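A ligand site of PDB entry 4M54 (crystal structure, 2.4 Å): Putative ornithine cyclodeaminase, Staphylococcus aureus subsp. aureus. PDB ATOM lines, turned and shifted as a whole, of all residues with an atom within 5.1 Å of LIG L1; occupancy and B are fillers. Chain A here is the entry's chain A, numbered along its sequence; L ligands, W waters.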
ATOM      1  N   ARG A  63      16.461 -14.390 -32.184  1.00  0.00           N
ATOM      2  CA  ARG A  63      15.399 -14.446 -31.187  1.00  0.00           C
ATOM      3  C   ARG A  63      15.657 -13.500 -30.022  1.00  0.00           C
ATOM      4  O   ARG A  63      16.766 -12.979 -29.870  1.00  0.00           O
ATOM      5  CB  ARG A  63      15.231 -15.868 -30.642  1.00  0.00           C
ATOM      6  CG  ARG A  63      16.318 -16.295 -29.654  1.00  0.00           C
ATOM      7  CD  ARG A  63      17.620 -16.660 -30.354  1.00  0.00           C
ATOM      8  NE  ARG A  63      18.767 -16.659 -29.438  1.00  0.00           N
ATOM      9  CZ  ARG A  63      19.319 -17.750 -28.932  1.00  0.00           C
ATOM     10  NH1 ARG A  63      18.839 -18.948 -29.234  1.00  0.00           N
ATOM     11  NH2 ARG A  63      20.362 -17.641 -28.114  1.00  0.00           N
ATOM     12  N   PRO A  90      27.226  -9.451 -36.100  1.00  0.00           N
ATOM     13  CA  PRO A  90      28.658  -9.223 -36.350  1.00  0.00           C
ATOM     14  C   PRO A  90      28.977  -9.212 -37.840  1.00  0.00           C
ATOM     15  O   PRO A  90      29.844  -8.433 -38.268  1.00  0.00           O
ATOM     16  CB  PRO A  90      29.325 -10.436 -35.687  1.00  0.00           C
ATOM     17  CG  PRO A  90      28.303 -10.992 -34.741  1.00  0.00           C
ATOM     18  CD  PRO A  90      26.986 -10.722 -35.408  1.00  0.00           C
ATOM     19  N   ARG A  97      26.376 -10.138 -31.575  1.00  0.00           N
ATOM     20  CA  ARG A  97      25.193 -10.955 -31.840  1.00  0.00           C
ATOM     21  C   ARG A  97      24.145 -10.762 -30.751  1.00  0.00           C
ATOM     22  O   ARG A  97      22.994 -10.450 -31.031  1.00  0.00           O
ATOM     23  CB  ARG A  97      25.577 -12.431 -31.924  1.00  0.00           C
ATOM     24  CG  ARG A  97      24.383 -13.368 -31.996  1.00  0.00           C
ATOM     25  CD  ARG A  97      24.772 -14.787 -31.635  1.00  0.00           C
ATOM     26  NE  ARG A  97      25.312 -14.867 -30.271  1.00  0.00           N
ATOM     27  CZ  ARG A  97      24.569 -15.067 -29.185  1.00  0.00           C
ATOM     28  NH1 ARG A  97      23.252 -15.217 -29.297  1.00  0.00           N
ATOM     29  NH2 ARG A  97      25.137 -15.128 -27.990  1.00  0.00           N
ATOM     30  N   SER A 122      25.980 -11.939 -19.111  1.00  0.00           N
ATOM     31  CA  SER A 122      25.562 -13.213 -19.698  1.00  0.00           C
ATOM     32  C   SER A 122      26.753 -14.069 -20.121  1.00  0.00           C
ATOM     33  O   SER A 122      26.816 -15.258 -19.816  1.00  0.00           O
ATOM     34  CB  SER A 122      24.635 -12.962 -20.899  1.00  0.00           C
ATOM     35  OG  SER A 122      24.169 -14.185 -21.452  1.00  0.00           O
ATOM     36  N   ARG A 125      28.914 -15.164 -16.891  1.00  0.00           N
ATOM     37  CA  ARG A 125      28.311 -16.189 -16.042  1.00  0.00           C
ATOM     38  C   ARG A 125      28.349 -17.546 -16.751  1.00  0.00           C
ATOM     39  O   ARG A 125      28.490 -18.587 -16.108  1.00  0.00           O
ATOM     40  CB  ARG A 125      26.881 -15.820 -15.621  1.00  0.00           C
ATOM     41  CG  ARG A 125      25.843 -15.652 -16.747  1.00  0.00           C
ATOM     42  CD  ARG A 125      25.163 -16.970 -17.124  1.00  0.00           C
ATOM     43  NE  ARG A 125      23.835 -16.756 -17.697  1.00  0.00           N
ATOM     44  CZ  ARG A 125      23.152 -17.685 -18.364  1.00  0.00           C
ATOM     45  NH1 ARG A 125      23.676 -18.877 -18.571  1.00  0.00           N
ATOM     46  NH2 ARG A 125      21.949 -17.406 -18.841  1.00  0.00           N
ATOM     47  N   THR A 126      28.251 -17.517 -18.080  1.00  0.00           N
ATOM     48  CA  THR A 126      28.311 -18.727 -18.882  1.00  0.00           C
ATOM     49  C   THR A 126      29.712 -19.336 -18.791  1.00  0.00           C
ATOM     50  O   THR A 126      29.868 -20.558 -18.733  1.00  0.00           O
ATOM     51  CB  THR A 126      27.972 -18.437 -20.349  1.00  0.00           C
ATOM     52  OG1 THR A 126      26.692 -17.804 -20.426  1.00  0.00           O
ATOM     53  CG2 THR A 126      27.945 -19.730 -21.155  1.00  0.00           C
ATOM     54  N   ILE A 148      36.023 -24.205 -29.444  1.00  0.00           N
ATOM     55  CA  ILE A 148      35.482 -24.172 -30.798  1.00  0.00           C
ATOM     56  C   ILE A 148      34.480 -23.032 -30.929  1.00  0.00           C
ATOM     57  O   ILE A 148      33.435 -23.028 -30.277  1.00  0.00           O
ATOM     58  CB  ILE A 148      34.812 -25.498 -31.211  1.00  0.00           C
ATOM     59  CG1 ILE A 148      35.800 -26.663 -31.084  1.00  0.00           C
ATOM     60  CG2 ILE A 148      34.305 -25.407 -32.641  1.00  0.00           C
ATOM     61  CD1 ILE A 148      35.692 -27.421 -29.794  1.00  0.00           C
ATOM     62  N   GLY A 149      34.802 -22.058 -31.776  1.00  0.00           N
ATOM     63  CA  GLY A 149      33.997 -20.866 -31.901  1.00  0.00           C
ATOM     64  C   GLY A 149      34.721 -19.687 -31.284  1.00  0.00           C
ATOM     65  O   GLY A 149      34.887 -19.613 -30.069  1.00  0.00           O
ATOM     66  N   CYS A 150      35.171 -18.769 -32.129  1.00  0.00           N
ATOM     67  CA  CYS A 150      35.984 -17.649 -31.682  1.00  0.00           C
ATOM     68  C   CYS A 150      35.186 -16.357 -31.594  1.00  0.00           C
ATOM     69  O   CYS A 150      35.698 -15.275 -31.895  1.00  0.00           O
ATOM     70  CB  CYS A 150      37.176 -17.466 -32.630  1.00  0.00           C
ATOM     71  SG  CYS A 150      38.194 -18.938 -32.787  1.00  0.00           S
ATOM     72  N   GLY A 151      33.924 -16.478 -31.193  1.00  0.00           N
ATOM     73  CA  GLY A 151      33.065 -15.325 -31.044  1.00  0.00           C
ATOM     74  C   GLY A 151      33.182 -14.691 -29.667  1.00  0.00           C
ATOM     75  O   GLY A 151      34.187 -14.863 -28.976  1.00  0.00           O
ATOM     76  N   LEU A 152      32.152 -13.960 -29.276  1.00  0.00           N
ATOM     77  CA  LEU A 152      32.148 -13.259 -27.994  1.00  0.00           C
ATOM     78  C   LEU A 152      32.167 -14.253 -26.831  1.00  0.00           C
ATOM     79  O   LEU A 152      32.975 -14.114 -25.906  1.00  0.00           O
ATOM     80  CB  LEU A 152      30.924 -12.351 -27.907  1.00  0.00           C
ATOM     81  CG  LEU A 152      30.874 -11.241 -26.849  1.00  0.00           C
ATOM     82  CD1 LEU A 152      30.401 -11.745 -25.495  1.00  0.00           C
ATOM     83  CD2 LEU A 152      32.233 -10.562 -26.727  1.00  0.00           C
ATOM     84  N   ILE A 153      31.282 -15.238 -26.883  1.00  0.00           N
ATOM     85  CA  ILE A 153      31.187 -16.246 -25.827  1.00  0.00           C
ATOM     86  C   ILE A 153      32.494 -17.016 -25.674  1.00  0.00           C
ATOM     87  O   ILE A 153      33.007 -17.157 -24.562  1.00  0.00           O
ATOM     88  CB  ILE A 153      30.031 -17.229 -26.097  1.00  0.00           C
ATOM     89  CG1 ILE A 153      28.679 -16.548 -25.885  1.00  0.00           C
ATOM     90  CG2 ILE A 153      30.140 -18.453 -25.190  1.00  0.00           C
ATOM     91  CD1 ILE A 153      28.401 -16.164 -24.450  1.00  0.00           C
ATOM     92  N   GLY A 154      33.029 -17.515 -26.790  1.00  0.00           N
ATOM     93  CA  GLY A 154      34.271 -18.269 -26.789  1.00  0.00           C
ATOM     94  C   GLY A 154      35.432 -17.499 -26.195  1.00  0.00           C
ATOM     95  O   GLY A 154      36.302 -18.069 -25.536  1.00  0.00           O
ATOM     96  N   TYR A 174      39.654 -23.609 -32.814  1.00  0.00           N
ATOM     97  CA  TYR A 174      39.149 -23.796 -34.168  1.00  0.00           C
ATOM     98  C   TYR A 174      37.866 -22.999 -34.414  1.00  0.00           C
ATOM     99  O   TYR A 174      37.011 -22.895 -33.533  1.00  0.00           O
ATOM    100  CB  TYR A 174      38.912 -25.275 -34.475  1.00  0.00           C
ATOM    101  CG  TYR A 174      38.279 -25.492 -35.833  1.00  0.00           C
ATOM    102  CD1 TYR A 174      39.038 -25.417 -36.995  1.00  0.00           C
ATOM    103  CD2 TYR A 174      36.919 -25.761 -35.965  1.00  0.00           C
ATOM    104  CE1 TYR A 174      38.464 -25.616 -38.245  1.00  0.00           C
ATOM    105  CE2 TYR A 174      36.334 -25.957 -37.201  1.00  0.00           C
ATOM    106  CZ  TYR A 174      37.117 -25.882 -38.337  1.00  0.00           C
ATOM    107  OH  TYR A 174      36.542 -26.075 -39.574  1.00  0.00           O
ATOM    108  N   ASP A 175      37.762 -22.453 -35.610  1.00  0.00           N
ATOM    109  CA  ASP A 175      36.539 -21.791 -36.059  1.00  0.00           C
ATOM    110  C   ASP A 175      36.332 -22.174 -37.523  1.00  0.00           C
ATOM    111  O   ASP A 175      37.300 -22.290 -38.282  1.00  0.00           O
ATOM    112  CB  ASP A 175      36.680 -20.275 -35.934  1.00  0.00           C
ATOM    113  CG  ASP A 175      35.325 -19.567 -35.946  1.00  0.00           C
ATOM    114  OD1 ASP A 175      34.733 -19.437 -37.035  1.00  0.00           O
ATOM    115  OD2 ASP A 175      34.876 -19.138 -34.864  1.00  0.00           O
ATOM    116  N   GLN A 176      35.074 -22.391 -37.915  1.00  0.00           N
ATOM    117  CA  GLN A 176      34.773 -22.763 -39.305  1.00  0.00           C
ATOM    118  C   GLN A 176      35.206 -21.653 -40.255  1.00  0.00           C
ATOM    119  O   GLN A 176      35.572 -21.902 -41.400  1.00  0.00           O
ATOM    120  CB  GLN A 176      33.278 -23.055 -39.469  1.00  0.00           C
ATOM    121  CG  GLN A 176      32.372 -21.860 -39.226  1.00  0.00           C
ATOM    122  CD  GLN A 176      30.912 -22.167 -39.516  1.00  0.00           C
ATOM    123  OE1 GLN A 176      30.503 -23.322 -39.602  1.00  0.00           O
ATOM    124  NE2 GLN A 176      30.111 -21.115 -39.678  1.00  0.00           N
ATOM    125  N   PHE A 177      35.168 -20.415 -39.755  1.00  0.00           N
ATOM    126  CA  PHE A 177      35.642 -19.270 -40.495  1.00  0.00           C
ATOM    127  C   PHE A 177      37.111 -19.053 -40.124  1.00  0.00           C
ATOM    128  O   PHE A 177      37.408 -18.579 -39.023  1.00  0.00           O
ATOM    129  CB  PHE A 177      34.800 -18.045 -40.142  1.00  0.00           C
ATOM    130  CG  PHE A 177      35.152 -16.815 -40.930  1.00  0.00           C
ATOM    131  CD1 PHE A 177      35.752 -16.912 -42.168  1.00  0.00           C
ATOM    132  CD2 PHE A 177      34.875 -15.564 -40.410  1.00  0.00           C
ATOM    133  CE1 PHE A 177      36.060 -15.775 -42.886  1.00  0.00           C
ATOM    134  CE2 PHE A 177      35.191 -14.417 -41.118  1.00  0.00           C
ATOM    135  CZ  PHE A 177      35.785 -14.526 -42.357  1.00  0.00           C
ATOM    136  N   ALA A 180      38.332 -15.786 -38.489  1.00  0.00           N
ATOM    137  CA  ALA A 180      37.884 -15.621 -37.096  1.00  0.00           C
ATOM    138  C   ALA A 180      38.847 -16.332 -36.145  1.00  0.00           C
ATOM    139  O   ALA A 180      39.141 -15.830 -35.067  1.00  0.00           O
ATOM    140  CB  ALA A 180      36.472 -16.158 -36.929  1.00  0.00           C
ATOM    141  N   CYS A 216      31.567 -23.225 -28.482  1.00  0.00           N
ATOM    142  CA  CYS A 216      30.999 -21.879 -28.458  1.00  0.00           C
ATOM    143  C   CYS A 216      30.636 -21.417 -29.866  1.00  0.00           C
ATOM    144  O   CYS A 216      31.028 -20.335 -30.290  1.00  0.00           O
ATOM    145  CB  CYS A 216      31.991 -20.901 -27.830  1.00  0.00           C
ATOM    146  SG  CYS A 216      32.801 -21.505 -26.338  1.00  0.00           S
ATOM    147  N   THR A 217      29.866 -22.238 -30.582  1.00  0.00           N
ATOM    148  CA  THR A 217      29.466 -21.893 -31.938  1.00  0.00           C
ATOM    149  C   THR A 217      27.995 -21.519 -31.991  1.00  0.00           C
ATOM    150  O   THR A 217      27.360 -21.326 -30.953  1.00  0.00           O
ATOM    151  CB  THR A 217      29.709 -23.067 -32.905  1.00  0.00           C
ATOM    152  OG1 THR A 217      28.730 -24.089 -32.663  1.00  0.00           O
ATOM    153  CG2 THR A 217      31.102 -23.648 -32.700  1.00  0.00           C
ATOM    154  N   VAL A 218      27.452 -21.412 -33.200  1.00  0.00           N
ATOM    155  CA  VAL A 218      26.028 -21.146 -33.384  1.00  0.00           C
ATOM    156  C   VAL A 218      25.454 -22.210 -34.306  1.00  0.00           C
ATOM    157  O   VAL A 218      24.466 -21.971 -35.015  1.00  0.00           O
ATOM    158  CB  VAL A 218      25.783 -19.755 -33.991  1.00  0.00           C
ATOM    159  CG1 VAL A 218      26.123 -18.667 -32.973  1.00  0.00           C
ATOM    160  CG2 VAL A 218      26.576 -19.576 -35.270  1.00  0.00           C
ATOM    161  N   THR A 219      26.069 -23.385 -34.296  1.00  0.00           N
ATOM    162  CA  THR A 219      25.687 -24.469 -35.199  1.00  0.00           C
ATOM    163  C   THR A 219      24.341 -25.100 -34.837  1.00  0.00           C
ATOM    164  O   THR A 219      23.852 -24.961 -33.717  1.00  0.00           O
ATOM    165  CB  THR A 219      26.771 -25.573 -35.265  1.00  0.00           C
ATOM    166  OG1 THR A 219      26.520 -26.435 -36.379  1.00  0.00           O
ATOM    167  CG2 THR A 219      26.780 -26.389 -33.981  1.00  0.00           C
ATOM    168  N   TYR A 223      28.747 -32.258 -34.697  1.00  0.00           N
ATOM    169  CA  TYR A 223      29.925 -32.681 -35.450  1.00  0.00           C
ATOM    170  C   TYR A 223      30.896 -33.423 -34.529  1.00  0.00           C
ATOM    171  O   TYR A 223      31.742 -34.194 -34.988  1.00  0.00           O
ATOM    172  CB  TYR A 223      30.633 -31.470 -36.083  1.00  0.00           C
ATOM    173  CG  TYR A 223      30.953 -30.367 -35.100  1.00  0.00           C
ATOM    174  CD1 TYR A 223      32.163 -30.345 -34.422  1.00  0.00           C
ATOM    175  CD2 TYR A 223      30.046 -29.347 -34.860  1.00  0.00           C
ATOM    176  CE1 TYR A 223      32.458 -29.345 -33.523  1.00  0.00           C
ATOM    177  CE2 TYR A 223      30.329 -28.341 -33.957  1.00  0.00           C
ATOM    178  CZ  TYR A 223      31.537 -28.348 -33.296  1.00  0.00           C
ATOM    179  OH  TYR A 223      31.829 -27.338 -32.394  1.00  0.00           O
ATOM    180  N   ILE A 238      28.593 -25.673 -24.252  1.00  0.00           N
ATOM    181  CA  ILE A 238      27.939 -24.376 -24.097  1.00  0.00           C
ATOM    182  C   ILE A 238      26.928 -24.079 -25.218  1.00  0.00           C
ATOM    183  O   ILE A 238      25.808 -23.661 -24.940  1.00  0.00           O
ATOM    184  CB  ILE A 238      28.981 -23.232 -24.037  1.00  0.00           C
ATOM    185  CG1 ILE A 238      29.864 -23.380 -22.790  1.00  0.00           C
ATOM    186  CG2 ILE A 238      28.296 -21.870 -24.048  1.00  0.00           C
ATOM    187  CD1 ILE A 238      29.095 -23.328 -21.488  1.00  0.00           C
ATOM    188  N   SER A 239      27.333 -24.316 -26.462  1.00  0.00           N
ATOM    189  CA  SER A 239      26.464 -24.032 -27.603  1.00  0.00           C
ATOM    190  C   SER A 239      25.490 -25.171 -27.918  1.00  0.00           C
ATOM    191  O   SER A 239      24.796 -25.121 -28.933  1.00  0.00           O
ATOM    192  CB  SER A 239      27.295 -23.648 -28.828  1.00  0.00           C
ATOM    193  OG  SER A 239      28.375 -24.545 -29.030  1.00  0.00           O
ATOM    194  N   ILE A 240      25.471 -26.180 -27.057  1.00  0.00           N
ATOM    195  CA  ILE A 240      24.427 -27.212 -27.057  1.00  0.00           C
ATOM    196  C   ILE A 240      24.394 -28.144 -28.275  1.00  0.00           C
ATOM    197  O   ILE A 240      24.433 -29.371 -28.121  1.00  0.00           O
ATOM    198  CB  ILE A 240      23.014 -26.604 -26.851  1.00  0.00           C
ATOM    199  CG1 ILE A 240      22.942 -25.896 -25.491  1.00  0.00           C
ATOM    200  CG2 ILE A 240      21.940 -27.670 -26.949  1.00  0.00           C
ATOM    201  CD1 ILE A 240      23.150 -26.820 -24.317  1.00  0.00           C
ATOM    202  N   PRO A 309      24.645 -27.575 -20.436  1.00  0.00           N
ATOM    203  CA  PRO A 309      23.998 -26.461 -19.740  1.00  0.00           C
ATOM    204  C   PRO A 309      23.137 -25.607 -20.654  1.00  0.00           C
ATOM    205  O   PRO A 309      23.654 -24.946 -21.557  1.00  0.00           O
ATOM    206  CB  PRO A 309      25.193 -25.656 -19.218  1.00  0.00           C
ATOM    207  CG  PRO A 309      26.348 -26.008 -20.147  1.00  0.00           C
ATOM    208  CD  PRO A 309      25.927 -27.156 -21.027  1.00  0.00           C
ATOM    209  N   MET A 310      21.827 -25.621 -20.427  1.00  0.00           N
ATOM    210  CA  MET A 310      20.908 -24.806 -21.214  1.00  0.00           C
ATOM    211  C   MET A 310      21.014 -23.326 -20.838  1.00  0.00           C
ATOM    212  O   MET A 310      20.683 -22.454 -21.633  1.00  0.00           O
ATOM    213  CB  MET A 310      19.468 -25.291 -21.028  1.00  0.00           C
ATOM    214  CG  MET A 310      18.853 -25.927 -22.264  1.00  0.00           C
ATOM    215  SD  MET A 310      19.718 -27.415 -22.804  1.00  0.00           S
ATOM    216  CE  MET A 310      18.704 -27.889 -24.203  1.00  0.00           C
ATOM    217  N   GLY A 311      21.485 -23.061 -19.625  1.00  0.00           N
ATOM    218  CA  GLY A 311      21.575 -21.705 -19.121  1.00  0.00           C
ATOM    219  C   GLY A 311      20.346 -21.356 -18.293  1.00  0.00           C
ATOM    220  O   GLY A 311      19.212 -21.523 -18.749  1.00  0.00           O
ATOM    221  N   GLU A 315      21.197 -17.686 -12.803  1.00  0.00           N
ATOM    222  CA  GLU A 315      22.616 -17.411 -13.006  1.00  0.00           C
ATOM    223  C   GLU A 315      22.832 -15.942 -13.339  1.00  0.00           C
ATOM    224  O   GLU A 315      23.777 -15.316 -12.865  1.00  0.00           O
ATOM    225  CB  GLU A 315      23.183 -18.286 -14.119  1.00  0.00           C
ATOM    226  CG  GLU A 315      23.068 -19.786 -13.857  1.00  0.00           C
ATOM    227  CD  GLU A 315      23.493 -20.618 -15.046  1.00  0.00           C
ATOM    228  OE1 GLU A 315      23.536 -20.069 -16.166  1.00  0.00           O
ATOM    229  OE2 GLU A 315      23.794 -21.814 -14.853  1.00  0.00           O
HETATM  230  P1  LIG L   1      29.131 -15.299 -32.301  1.00  0.00           P
HETATM  231  O1  LIG L   1      28.292 -15.307 -33.564  1.00  0.00           O
HETATM  232  O2  LIG L   1      29.867 -13.978 -32.186  1.00  0.00           O
HETATM  233  O3  LIG L   1      30.173 -16.513 -32.344  1.00  0.00           O
HETATM  234  C1  LIG L   1      29.999 -17.499 -33.368  1.00  0.00           C
HETATM  235  C2  LIG L   1      31.339 -17.986 -33.823  1.00  0.00           C
HETATM  236  O4  LIG L   1      31.348 -19.467 -33.833  1.00  0.00           O
HETATM  237  C3  LIG L   1      31.598 -17.515 -35.195  1.00  0.00           C
HETATM  238  O5  LIG L   1      32.979 -17.076 -35.297  1.00  0.00           O
HETATM  239  C4  LIG L   1      31.387 -18.676 -36.057  1.00  0.00           C
HETATM  240  O6  LIG L   1      32.204 -18.593 -37.250  1.00  0.00           O
HETATM  241  C5  LIG L   1      31.804 -19.797 -35.216  1.00  0.00           C
HETATM  242  N1  LIG L   1      31.260 -21.006 -35.656  1.00  0.00           N
HETATM  243  C6  LIG L   1      30.039 -21.245 -36.081  1.00  0.00           C
HETATM  244  N2  LIG L   1      29.679 -22.258 -36.424  1.00  0.00           N
HETATM  245  C7  LIG L   1      30.354 -23.158 -36.420  1.00  0.00           C
HETATM  246  C8  LIG L   1      30.677 -24.596 -36.649  1.00  0.00           C
HETATM  247  N3  LIG L   1      29.608 -25.418 -37.159  1.00  0.00           N
HETATM  248  N4  LIG L   1      31.753 -25.163 -36.441  1.00  0.00           N
HETATM  249  C9  LIG L   1      32.707 -24.667 -36.033  1.00  0.00           C
HETATM  250  N5  LIG L   1      32.829 -23.487 -35.737  1.00  0.00           N
HETATM  251  C10 LIG L   1      31.810 -22.521 -35.824  1.00  0.00           C
HETATM  252  O7  LIG L   1      28.172 -15.446 -31.053  1.00  0.00           O
HETATM  253  P2  LIG L   1      28.662 -15.860 -29.596  1.00  0.00           P
HETATM  254  O8  LIG L   1      27.975 -14.955 -28.598  1.00  0.00           O
HETATM  255  O9  LIG L   1      30.167 -15.720 -29.462  1.00  0.00           O
HETATM  256  O10 LIG L   1      28.263 -17.397 -29.307  1.00  0.00           O
HETATM  257  C11 LIG L   1      26.935 -17.645 -28.852  1.00  0.00           C
HETATM  258  C12 LIG L   1      26.676 -19.106 -28.792  1.00  0.00           C
HETATM  259  O11 LIG L   1      26.856 -19.595 -27.387  1.00  0.00           O
HETATM  260  C13 LIG L   1      25.284 -19.336 -29.182  1.00  0.00           C
HETATM  261  O12 LIG L   1      25.158 -20.635 -29.833  1.00  0.00           O
HETATM  262  C14 LIG L   1      24.552 -19.341 -27.933  1.00  0.00           C
HETATM  263  O13 LIG L   1      23.279 -20.053 -28.070  1.00  0.00           O
HETATM  264  C15 LIG L   1      25.465 -20.045 -27.023  1.00  0.00           C
HETATM  265  N6  LIG L   1      25.157 -19.782 -25.686  1.00  0.00           N
HETATM  266  C16 LIG L   1      24.793 -20.577 -24.617  1.00  0.00           C
HETATM  267  C17 LIG L   1      24.708 -20.065 -23.346  1.00  0.00           C
HETATM  268  C18 LIG L   1      24.290 -21.024 -22.234  1.00  0.00           C
HETATM  269  O14 LIG L   1      23.916 -20.594 -21.146  1.00  0.00           O
HETATM  270  N7  LIG L   1      24.344 -22.430 -22.465  1.00  0.00           N
HETATM  271  C19 LIG L   1      25.034 -18.555 -23.007  1.00  0.00           C
HETATM  272  C20 LIG L   1      25.205 -17.775 -24.335  1.00  0.00           C
HETATM  273  C21 LIG L   1      25.265 -18.383 -25.573  1.00  0.00           C
HETATM  274  O1  LG2 L   2      23.505 -14.801 -25.794  1.00  0.00           O
HETATM  275  C1  LG2 L   2      22.448 -15.466 -25.647  1.00  0.00           C
HETATM  276  O2  LG2 L   2      21.665 -15.627 -26.613  1.00  0.00           O
HETATM  277  C2  LG2 L   2      22.134 -16.082 -24.290  1.00  0.00           C
HETATM  278  C3  LG2 L   2      20.990 -17.053 -24.413  1.00  0.00           C
HETATM  279  C4  LG2 L   2      21.271 -18.289 -23.532  1.00  0.00           C
HETATM  280  N1  LG2 L   2      20.407 -19.338 -23.909  1.00  0.00           N
HETATM  281  C5  LG2 L   2      20.943 -19.997 -25.076  1.00  0.00           C
HETATM  282  C6  LG2 L   2      20.306 -21.390 -25.208  1.00  0.00           C
HETATM  283  N2  LG2 L   2      21.249 -22.376 -24.795  1.00  0.00           N
HETATM  284  C7  LG2 L   2      19.922 -21.639 -26.655  1.00  0.00           C
HETATM  285  O3  LG2 L   2      18.881 -21.104 -27.141  1.00  0.00           O
HETATM  286  O4  LG2 L   2      20.632 -22.376 -27.362  1.00  0.00           O
HETATM  287  C8  LG2 L   2      21.047 -17.958 -22.079  1.00  0.00           C
HETATM  288  O5  LG2 L   2      20.971 -18.898 -21.220  1.00  0.00           O
HETATM  289  O6  LG2 L   2      20.942 -16.749 -21.699  1.00  0.00           O
HETATM  290  O   HOH W   1      32.141 -17.996 -29.551  1.00  0.00           O
HETATM  291  O   HOH W   2      29.251 -11.606 -30.978  1.00  0.00           O
HETATM  292  O   HOH W   3      33.241 -27.688 -36.328  1.00  0.00           O
HETATM  293  O   HOH W   4      27.258 -11.793 -28.724  1.00  0.00           O
HETATM  294  O   HOH W   5      26.064 -15.789 -35.037  1.00  0.00           O
HETATM  295  O   HOH W   6      23.632 -23.178 -31.329  1.00  0.00           O
HETATM  296  O   HOH W   7      27.348 -24.813 -38.582  1.00  0.00           O
HETATM  297  O   HOH W   8      25.235 -14.320 -23.875  1.00  0.00           O
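O1 of LG2 L2 lies within salt-bridge range of NH2 of Arg 97, at 2.8 Å. The backbone carbonyl oxygen of Pro 309 sits at hydrogen-bond distance from a nitrogen (N7) of LIG L1. NH1 of Arg 125 sits at hydrogen-bond distance from O14 of LIG L1 (3.1 Å). A nitrogen (N2) of LG2 L2 is in hydrogen-bond range of the backbone carbonyl oxygen (O) of Met 310 (3.2 Å). A nitrogen (N7) of LIG L1 is in hydrogen-bond range of the backbone carbonyl oxygen (O) of Ile 238 (3.1 Å). O2 of LG2 L2 is in salt-bridge range of NH2 of Arg 63, at 2.8 Å. The side-chain carboxylate (OD1) of Asp 175 lies within hydrogen-bond range of an oxygen (O6) of LIG L1 (2.7 Å). N of Ile 153 sits at hydrogen-bond distance from O9 of LIG L1 (2.9 Å). The side-chain amide oxygen (OE1) of Gln 176 lies close to a nitrogen (N3) of LIG L1. The guanidinium group of Arg 125 lies within salt-bridge range of an oxygen (O5) of LG2 L2, 3.0 Å away. N3 of LIG L1 lies within hydrogen-bond range of OG1 of Thr 219, 3.3 Å away. The guanidinium group (NH2) of Arg 97 is in salt-bridge range of an oxygen (O8) of LIG L1 (2.9 Å). The backbone NH of Gln 176 lies within hydrogen-bond range of a nitrogen (N5) of LIG L1 (3.3 Å). N of Leu 152 lies within hydrogen-bond range of O9 of LIG L1, 2.7 Å away. The backbone carbonyl oxygen (O) of Thr 217 is in hydrogen-bond range of an oxygen (O12) of LIG L1.
Residues that only touch LIG L1: Thr 126 (3.2 Å), Gly 151 (3.2 Å), Gly 311 (3.3 Å), Gly 149 (3.6 Å), Cys 216 (3.7 Å), Val 218 (3.7 Å), Met 310 (3.8 Å), Arg 63 (3.8 Å), Ile 148 (3.8 Å), Ser 239 (3.8 Å), Phe 177 (3.9 Å) and Ala 180 (3.96 Å). Within 4 Å of LIG L1: Arg 63, Arg 97, Arg 125, Thr 126, Ile 148, Gly 149, Gly 151, Leu 152, Ile 153, Asp 175, Gln 176, Phe 177, Ala 180, Cys 216, Thr 217, Val 218, Thr 219, Ile 238, Ser 239, Pro 309, Met 310 and Gly 311.
The backbone carbonyl oxygen of Ser 122 sits at hydrogen-bond distance from the side-chain hydroxyl of Thr 126 (2.6 Å). O of Ile 148 is in hydrogen-bond range of N of Cys 216 (2.6 Å). The side-chain carboxylate (OD1) of Asp 175 lies within hydrogen-bond range of the backbone NH (N) of Phe 177 (2.9 Å). The guanidinium group of Arg 125 lies within salt-bridge range of the side-chain carboxylate of Glu 315, 2.7 Å away. The backbone NH (N) of Thr 219 is in hydrogen-bond range of the side-chain hydroxyl (OG1) of Thr 217 (3.2 Å). The side-chain carboxylate (OD2) of Asp 175 lies within hydrogen-bond range of the backbone NH (N) of Cys 150, at 2.8 Å. The backbone NH (N) of Gly 149 lies within hydrogen-bond range of the backbone carbonyl oxygen (O) of Tyr 174. N of Cys 216 is in hydrogen-bond range of OG of Ser 239, 3.5 Å away.
Water W2 lies within hydrogen-bond range of an oxygen (O2) of LIG L1 (2.7 Å) and the backbone NH of Arg 97 (3.3 Å). Water W7 bridges a nitrogen (N3) of LIG L1 (2.7 Å) and the side-chain hydroxyl of Thr 219 (2.9 Å). Water W1 lies within hydrogen-bond range of O of Cys 216 (2.7 Å), N of Gly 151 (2.9 Å), N of Gly 154 (2.9 Å), O9 of LIG L1 (3.0 Å) and O of Gly 149 (3.2 Å). Water W4 lies within hydrogen-bond range of an oxygen (O8) of LIG L1 and the backbone NH of Arg 97. Water W6 lies within hydrogen-bond range of the backbone carbonyl oxygen (O) of Thr 219, the backbone carbonyl oxygen (O) of Ser 239 and an oxygen (O12) of LIG L1. Water W8 lies within hydrogen-bond range of O1 of LG2 L2 (2.6 Å) and OG of Ser 122 (2.7 Å).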
